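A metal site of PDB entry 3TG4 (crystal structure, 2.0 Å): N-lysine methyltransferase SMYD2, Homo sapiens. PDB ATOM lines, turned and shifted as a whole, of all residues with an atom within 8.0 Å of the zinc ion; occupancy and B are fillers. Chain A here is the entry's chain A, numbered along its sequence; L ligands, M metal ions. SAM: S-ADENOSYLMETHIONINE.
SG of Cys 262 is bound to the zinc ion.
The zinc ion is bound by the side-chain sulfur (SG) of Cys 267 (2.3 Å).
The side-chain sulfur (SG) of Cys 264 binds the zinc ion (2.3 Å).
SG of Cys 209 binds the zinc ion (2.4 Å).
The backbone NH of His 207 is in hydrogen-bond range of a nitrogen (N7) of the ligand.
O of His 207 is in hydrogen-bond range of N6 of the ligand (3.0 Å).
The backbone NH of Cys 262 sits close to the side-chain amide nitrogen of Asn 251 (2.9 Å).
The guanidinium group (NH2) of Arg 250 lies close to the side-chain sulfur (SG) of Cys 267 (3.3 Å).
SG of Cys 267 lies close to OD1 of Asn 251, at 3.5 Å.
The backbone NH (N) of Glu 266 lies close to the side-chain sulfur (SG) of Cys 264, at 3.3 Å.
The backbone carbonyl oxygen (O) of Cys 264 sits at hydrogen-bond distance from the side-chain hydroxyl (OG1) of Thr 268.
NE of Arg 250 lies close to SG of Cys 209 (3.3 Å).
Four residues have an atom within 4 Å of the zinc ion: Cys 209, Cys 262, Cys 264 and Cys 267.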
ATOM      1  N   HIS A 207      -5.138  17.935   5.113  1.00  0.00           N
ATOM      2  CA  HIS A 207      -6.180  18.806   4.588  1.00  0.00           C
ATOM      3  C   HIS A 207      -5.671  20.165   4.080  1.00  0.00           C
ATOM      4  O   HIS A 207      -4.675  20.717   4.592  1.00  0.00           O
ATOM      5  CB  HIS A 207      -7.261  19.039   5.649  1.00  0.00           C
ATOM      6  CG  HIS A 207      -8.237  20.118   5.266  1.00  0.00           C
ATOM      7  ND1 HIS A 207      -8.017  21.446   5.572  1.00  0.00           N
ATOM      8  CD2 HIS A 207      -9.390  20.078   4.568  1.00  0.00           C
ATOM      9  CE1 HIS A 207      -9.003  22.173   5.089  1.00  0.00           C
ATOM     10  NE2 HIS A 207      -9.851  21.370   4.464  1.00  0.00           N
ATOM     11  N   SER A 208      -6.374  20.690   3.078  1.00  0.00           N
ATOM     12  CA  SER A 208      -6.268  22.077   2.634  1.00  0.00           C
ATOM     13  C   SER A 208      -7.609  22.509   2.046  1.00  0.00           C
ATOM     14  O   SER A 208      -8.331  21.695   1.501  1.00  0.00           O
ATOM     15  CB  SER A 208      -5.186  22.231   1.577  1.00  0.00           C
ATOM     16  OG  SER A 208      -5.211  23.542   1.011  1.00  0.00           O
ATOM     17  N   CYS A 209      -7.941  23.797   2.176  1.00  0.00           N
ATOM     18  CA  CYS A 209      -9.164  24.333   1.583  1.00  0.00           C
ATOM     19  C   CYS A 209      -8.992  24.721   0.123  1.00  0.00           C
ATOM     20  O   CYS A 209      -9.943  25.133  -0.535  1.00  0.00           O
ATOM     21  CB  CYS A 209      -9.697  25.513   2.378  1.00  0.00           C
ATOM     22  SG  CYS A 209      -9.693  25.183   4.103  1.00  0.00           S
ATOM     23  N   CYS A 210      -7.777  24.585  -0.384  1.00  0.00           N
ATOM     24  CA  CYS A 210      -7.529  24.590  -1.820  1.00  0.00           C
ATOM     25  C   CYS A 210      -6.774  23.312  -2.175  1.00  0.00           C
ATOM     26  O   CYS A 210      -5.584  23.348  -2.499  1.00  0.00           O
ATOM     27  CB  CYS A 210      -6.816  25.849  -2.275  1.00  0.00           C
ATOM     28  SG  CYS A 210      -5.500  26.362  -1.179  1.00  0.00           S
ATOM     29  N   PRO A 211      -7.480  22.166  -2.105  1.00  0.00           N
ATOM     30  CA  PRO A 211      -6.877  20.863  -2.283  1.00  0.00           C
ATOM     31  C   PRO A 211      -6.355  20.650  -3.706  1.00  0.00           C
ATOM     32  O   PRO A 211      -6.883  21.235  -4.648  1.00  0.00           O
ATOM     33  CB  PRO A 211      -8.041  19.897  -1.985  1.00  0.00           C
ATOM     34  CG  PRO A 211      -9.262  20.665  -2.370  1.00  0.00           C
ATOM     35  CD  PRO A 211      -8.947  22.089  -2.026  1.00  0.00           C
ATOM     36  N   SER A 239      -9.510  18.020   0.655  1.00  0.00           N
ATOM     37  CA  SER A 239     -10.326  18.756   1.609  1.00  0.00           C
ATOM     38  C   SER A 239     -11.131  17.773   2.437  1.00  0.00           C
ATOM     39  O   SER A 239     -11.809  16.915   1.878  1.00  0.00           O
ATOM     40  CB  SER A 239     -11.299  19.709   0.940  1.00  0.00           C
ATOM     41  OG  SER A 239     -12.156  20.251   1.935  1.00  0.00           O
ATOM     42  N   ILE A 241     -13.557  18.790   4.377  1.00  0.00           N
ATOM     43  CA  ILE A 241     -14.849  19.420   4.670  1.00  0.00           C
ATOM     44  C   ILE A 241     -15.536  20.033   3.453  1.00  0.00           C
ATOM     45  O   ILE A 241     -14.922  20.178   2.393  1.00  0.00           O
ATOM     46  CB  ILE A 241     -14.706  20.534   5.749  1.00  0.00           C
ATOM     47  CG1 ILE A 241     -13.421  21.341   5.509  1.00  0.00           C
ATOM     48  CG2 ILE A 241     -14.710  19.960   7.153  1.00  0.00           C
ATOM     49  CD1 ILE A 241     -13.558  22.807   5.866  1.00  0.00           C
ATOM     50  N   LEU A 243     -16.409  22.864   1.253  1.00  0.00           N
ATOM     51  CA  LEU A 243     -15.651  24.087   0.990  1.00  0.00           C
ATOM     52  C   LEU A 243     -16.491  25.336   0.710  1.00  0.00           C
ATOM     53  O   LEU A 243     -15.952  26.400   0.410  1.00  0.00           O
ATOM     54  CB  LEU A 243     -14.633  23.859  -0.142  1.00  0.00           C
ATOM     55  CG  LEU A 243     -13.523  22.837   0.165  1.00  0.00           C
ATOM     56  CD1 LEU A 243     -12.618  22.672  -1.050  1.00  0.00           C
ATOM     57  CD2 LEU A 243     -12.725  23.225   1.436  1.00  0.00           C
ATOM     58  N   THR A 247     -14.238  31.158   6.178  1.00  0.00           N
ATOM     59  CA  THR A 247     -13.021  30.671   6.840  1.00  0.00           C
ATOM     60  C   THR A 247     -13.240  30.248   8.304  1.00  0.00           C
ATOM     61  O   THR A 247     -12.750  29.201   8.735  1.00  0.00           O
ATOM     62  CB  THR A 247     -11.868  31.698   6.727  1.00  0.00           C
ATOM     63  OG1 THR A 247     -11.524  31.878   5.340  1.00  0.00           O
ATOM     64  CG2 THR A 247     -10.630  31.230   7.470  1.00  0.00           C
ATOM     65  N   ARG A 250     -15.416  26.902   8.415  1.00  0.00           N
ATOM     66  CA  ARG A 250     -14.569  25.759   8.043  1.00  0.00           C
ATOM     67  C   ARG A 250     -13.691  25.365   9.228  1.00  0.00           C
ATOM     68  O   ARG A 250     -13.669  24.200   9.642  1.00  0.00           O
ATOM     69  CB  ARG A 250     -13.665  26.099   6.849  1.00  0.00           C
ATOM     70  CG  ARG A 250     -14.411  26.462   5.564  1.00  0.00           C
ATOM     71  CD  ARG A 250     -13.519  26.290   4.319  1.00  0.00           C
ATOM     72  NE  ARG A 250     -12.303  27.123   4.311  1.00  0.00           N
ATOM     73  CZ  ARG A 250     -12.271  28.423   4.041  1.00  0.00           C
ATOM     74  NH1 ARG A 250     -13.397  29.088   3.788  1.00  0.00           N
ATOM     75  NH2 ARG A 250     -11.113  29.087   4.038  1.00  0.00           N
ATOM     76  N   ASN A 251     -13.015  26.350   9.817  1.00  0.00           N
ATOM     77  CA  ASN A 251     -12.079  26.081  10.897  1.00  0.00           C
ATOM     78  C   ASN A 251     -12.693  25.628  12.220  1.00  0.00           C
ATOM     79  O   ASN A 251     -12.079  24.833  12.942  1.00  0.00           O
ATOM     80  CB  ASN A 251     -11.110  27.242  11.091  1.00  0.00           C
ATOM     81  CG  ASN A 251      -9.980  27.195  10.109  1.00  0.00           C
ATOM     82  OD1 ASN A 251      -9.870  28.034   9.217  1.00  0.00           O
ATOM     83  ND2 ASN A 251      -9.132  26.183  10.248  1.00  0.00           N
ATOM     84  N   LEU A 254     -13.098  22.062  11.522  1.00  0.00           N
ATOM     85  CA  LEU A 254     -11.780  21.391  11.556  1.00  0.00           C
ATOM     86  C   LEU A 254     -11.212  21.221  12.981  1.00  0.00           C
ATOM     87  O   LEU A 254     -10.649  20.180  13.298  1.00  0.00           O
ATOM     88  CB  LEU A 254     -10.769  22.113  10.654  1.00  0.00           C
ATOM     89  CG  LEU A 254     -11.064  22.122   9.149  1.00  0.00           C
ATOM     90  CD1 LEU A 254     -10.071  22.992   8.456  1.00  0.00           C
ATOM     91  CD2 LEU A 254     -11.053  20.704   8.543  1.00  0.00           C
ATOM     92  N   PHE A 260      -7.324  20.603  14.505  1.00  0.00           N
ATOM     93  CA  PHE A 260      -6.337  21.539  13.966  1.00  0.00           C
ATOM     94  C   PHE A 260      -7.007  22.765  13.377  1.00  0.00           C
ATOM     95  O   PHE A 260      -8.214  22.737  13.069  1.00  0.00           O
ATOM     96  CB  PHE A 260      -5.417  20.857  12.930  1.00  0.00           C
ATOM     97  CG  PHE A 260      -6.086  20.583  11.602  1.00  0.00           C
ATOM     98  CD1 PHE A 260      -5.927  21.474  10.545  1.00  0.00           C
ATOM     99  CD2 PHE A 260      -6.874  19.441  11.411  1.00  0.00           C
ATOM    100  CE1 PHE A 260      -6.535  21.232   9.313  1.00  0.00           C
ATOM    101  CE2 PHE A 260      -7.481  19.199  10.179  1.00  0.00           C
ATOM    102  CZ  PHE A 260      -7.313  20.109   9.133  1.00  0.00           C
ATOM    103  N   THR A 261      -6.219  23.828  13.239  1.00  0.00           N
ATOM    104  CA  THR A 261      -6.585  24.996  12.455  1.00  0.00           C
ATOM    105  C   THR A 261      -5.765  24.998  11.156  1.00  0.00           C
ATOM    106  O   THR A 261      -4.538  24.832  11.165  1.00  0.00           O
ATOM    107  CB  THR A 261      -6.333  26.324  13.228  1.00  0.00           C
ATOM    108  OG1 THR A 261      -7.059  26.311  14.468  1.00  0.00           O
ATOM    109  CG2 THR A 261      -6.762  27.541  12.411  1.00  0.00           C
ATOM    110  N   CYS A 262      -6.461  25.186  10.042  1.00  0.00           N
ATOM    111  CA  CYS A 262      -5.840  25.200   8.727  1.00  0.00           C
ATOM    112  C   CYS A 262      -5.203  26.547   8.441  1.00  0.00           C
ATOM    113  O   CYS A 262      -5.769  27.602   8.783  1.00  0.00           O
ATOM    114  CB  CYS A 262      -6.862  24.879   7.649  1.00  0.00           C
ATOM    115  SG  CYS A 262      -6.181  24.814   5.984  1.00  0.00           S
ATOM    116  N   GLU A 263      -4.038  26.505   7.824  1.00  0.00           N
ATOM    117  CA  GLU A 263      -3.331  27.725   7.425  1.00  0.00           C
ATOM    118  C   GLU A 263      -3.033  27.725   5.919  1.00  0.00           C
ATOM    119  O   GLU A 263      -1.992  28.222   5.482  1.00  0.00           O
ATOM    120  CB  GLU A 263      -2.062  27.907   8.267  1.00  0.00           C
ATOM    121  CG  GLU A 263      -2.335  27.949   9.776  1.00  0.00           C
ATOM    122  CD  GLU A 263      -1.071  27.955  10.634  1.00  0.00           C
ATOM    123  OE1 GLU A 263       0.042  28.170  10.093  1.00  0.00           O
ATOM    124  OE2 GLU A 263      -1.203  27.762  11.859  1.00  0.00           O
ATOM    125  N   CYS A 264      -3.949  27.166   5.126  1.00  0.00           N
ATOM    126  CA  CYS A 264      -3.815  27.223   3.665  1.00  0.00           C
ATOM    127  C   CYS A 264      -3.991  28.662   3.154  1.00  0.00           C
ATOM    128  O   CYS A 264      -4.356  29.557   3.930  1.00  0.00           O
ATOM    129  CB  CYS A 264      -4.808  26.282   2.974  1.00  0.00           C
ATOM    130  SG  CYS A 264      -6.510  26.896   2.845  1.00  0.00           S
ATOM    131  N   GLN A 265      -3.748  28.867   1.860  1.00  0.00           N
ATOM    132  CA  GLN A 265      -3.896  30.186   1.225  1.00  0.00           C
ATOM    133  C   GLN A 265      -5.331  30.723   1.376  1.00  0.00           C
ATOM    134  O   GLN A 265      -5.512  31.908   1.608  1.00  0.00           O
ATOM    135  CB  GLN A 265      -3.483  30.123  -0.250  1.00  0.00           C
ATOM    136  CG  GLN A 265      -3.526  31.441  -0.996  1.00  0.00           C
ATOM    137  CD  GLN A 265      -2.183  32.138  -1.088  1.00  0.00           C
ATOM    138  OE1 GLN A 265      -1.419  32.204  -0.114  1.00  0.00           O
ATOM    139  NE2 GLN A 265      -1.885  32.677  -2.271  1.00  0.00           N
ATOM    140  N   GLU A 266      -6.330  29.845   1.299  1.00  0.00           N
ATOM    141  CA  GLU A 266      -7.733  30.275   1.430  1.00  0.00           C
ATOM    142  C   GLU A 266      -8.058  30.810   2.824  1.00  0.00           C
ATOM    143  O   GLU A 266      -8.779  31.810   2.969  1.00  0.00           O
ATOM    144  CB  GLU A 266      -8.713  29.142   1.058  1.00  0.00           C
ATOM    145  CG  GLU A 266      -8.585  28.591  -0.366  1.00  0.00           C
ATOM    146  CD  GLU A 266      -9.073  29.551  -1.455  1.00  0.00           C
ATOM    147  OE1 GLU A 266      -9.537  30.690  -1.181  1.00  0.00           O
ATOM    148  OE2 GLU A 266      -8.959  29.154  -2.639  1.00  0.00           O
ATOM    149  N   CYS A 267      -7.498  30.154   3.842  1.00  0.00           N
ATOM    150  CA  CYS A 267      -7.767  30.492   5.229  1.00  0.00           C
ATOM    151  C   CYS A 267      -6.901  31.697   5.651  1.00  0.00           C
ATOM    152  O   CYS A 267      -7.334  32.528   6.461  1.00  0.00           O
ATOM    153  CB  CYS A 267      -7.577  29.263   6.147  1.00  0.00           C
ATOM    154  SG  CYS A 267      -8.763  27.841   5.912  1.00  0.00           S
ATOM    155  N   THR A 268      -5.696  31.804   5.089  1.00  0.00           N
ATOM    156  CA  THR A 268      -4.792  32.954   5.313  1.00  0.00           C
ATOM    157  C   THR A 268      -5.329  34.264   4.733  1.00  0.00           C
ATOM    158  O   THR A 268      -5.359  35.300   5.420  1.00  0.00           O
ATOM    159  CB  THR A 268      -3.383  32.711   4.717  1.00  0.00           C
ATOM    160  OG1 THR A 268      -2.861  31.476   5.197  1.00  0.00           O
ATOM    161  CG2 THR A 268      -2.417  33.856   5.072  1.00  0.00           C
HETATM  162  N   SAM L   1      -1.430  13.934   9.739  1.00  0.00           N
HETATM  163  CA  SAM L   1      -2.092  12.600   9.868  1.00  0.00           C
HETATM  164  C   SAM L   1      -1.138  11.537  10.390  1.00  0.00           C
HETATM  165  O   SAM L   1      -1.510  10.352  10.541  1.00  0.00           O
HETATM  166  OXT SAM L   1       0.035  11.817  10.689  1.00  0.00           O
HETATM  167  CB  SAM L   1      -2.719  12.158   8.539  1.00  0.00           C
HETATM  168  CG  SAM L   1      -4.070  12.829   8.285  1.00  0.00           C
HETATM  169  SD  SAM L   1      -5.338  12.298   9.474  1.00  0.00           S
HETATM  170  CE  SAM L   1      -6.664  11.813   8.332  1.00  0.00           C
HETATM  171  C5' SAM L   1      -6.072  13.819  10.106  1.00  0.00           C
HETATM  172  C4' SAM L   1      -5.132  14.557  11.074  1.00  0.00           C
HETATM  173  O4' SAM L   1      -3.988  15.091  10.410  1.00  0.00           O
HETATM  174  C3' SAM L   1      -5.793  15.749  11.708  1.00  0.00           C
HETATM  175  O3' SAM L   1      -6.529  15.376  12.838  1.00  0.00           O
HETATM  176  C2' SAM L   1      -4.621  16.651  12.065  1.00  0.00           C
HETATM  177  O2' SAM L   1      -4.040  16.237  13.299  1.00  0.00           O
HETATM  178  C1' SAM L   1      -3.653  16.363  10.955  1.00  0.00           C
HETATM  179  N9  SAM L   1      -3.739  17.384   9.876  1.00  0.00           N
HETATM  180  C8  SAM L   1      -4.262  17.175   8.624  1.00  0.00           C
HETATM  181  N7  SAM L   1      -4.163  18.318   7.921  1.00  0.00           N
HETATM  182  C5  SAM L   1      -3.576  19.263   8.693  1.00  0.00           C
HETATM  183  C6  SAM L   1      -3.247  20.599   8.459  1.00  0.00           C
HETATM  184  N6  SAM L   1      -3.513  21.150   7.272  1.00  0.00           N
HETATM  185  N1  SAM L   1      -2.660  21.345   9.458  1.00  0.00           N
HETATM  186  C2  SAM L   1      -2.394  20.766  10.692  1.00  0.00           C
HETATM  187  N3  SAM L   1      -2.715  19.433  10.915  1.00  0.00           N
HETATM  188  C4  SAM L   1      -3.300  18.694   9.937  1.00  0.00           C
HETATM  189 ZN    ZN M   1      -7.638  26.151   4.757  1.00  0.00          ZN
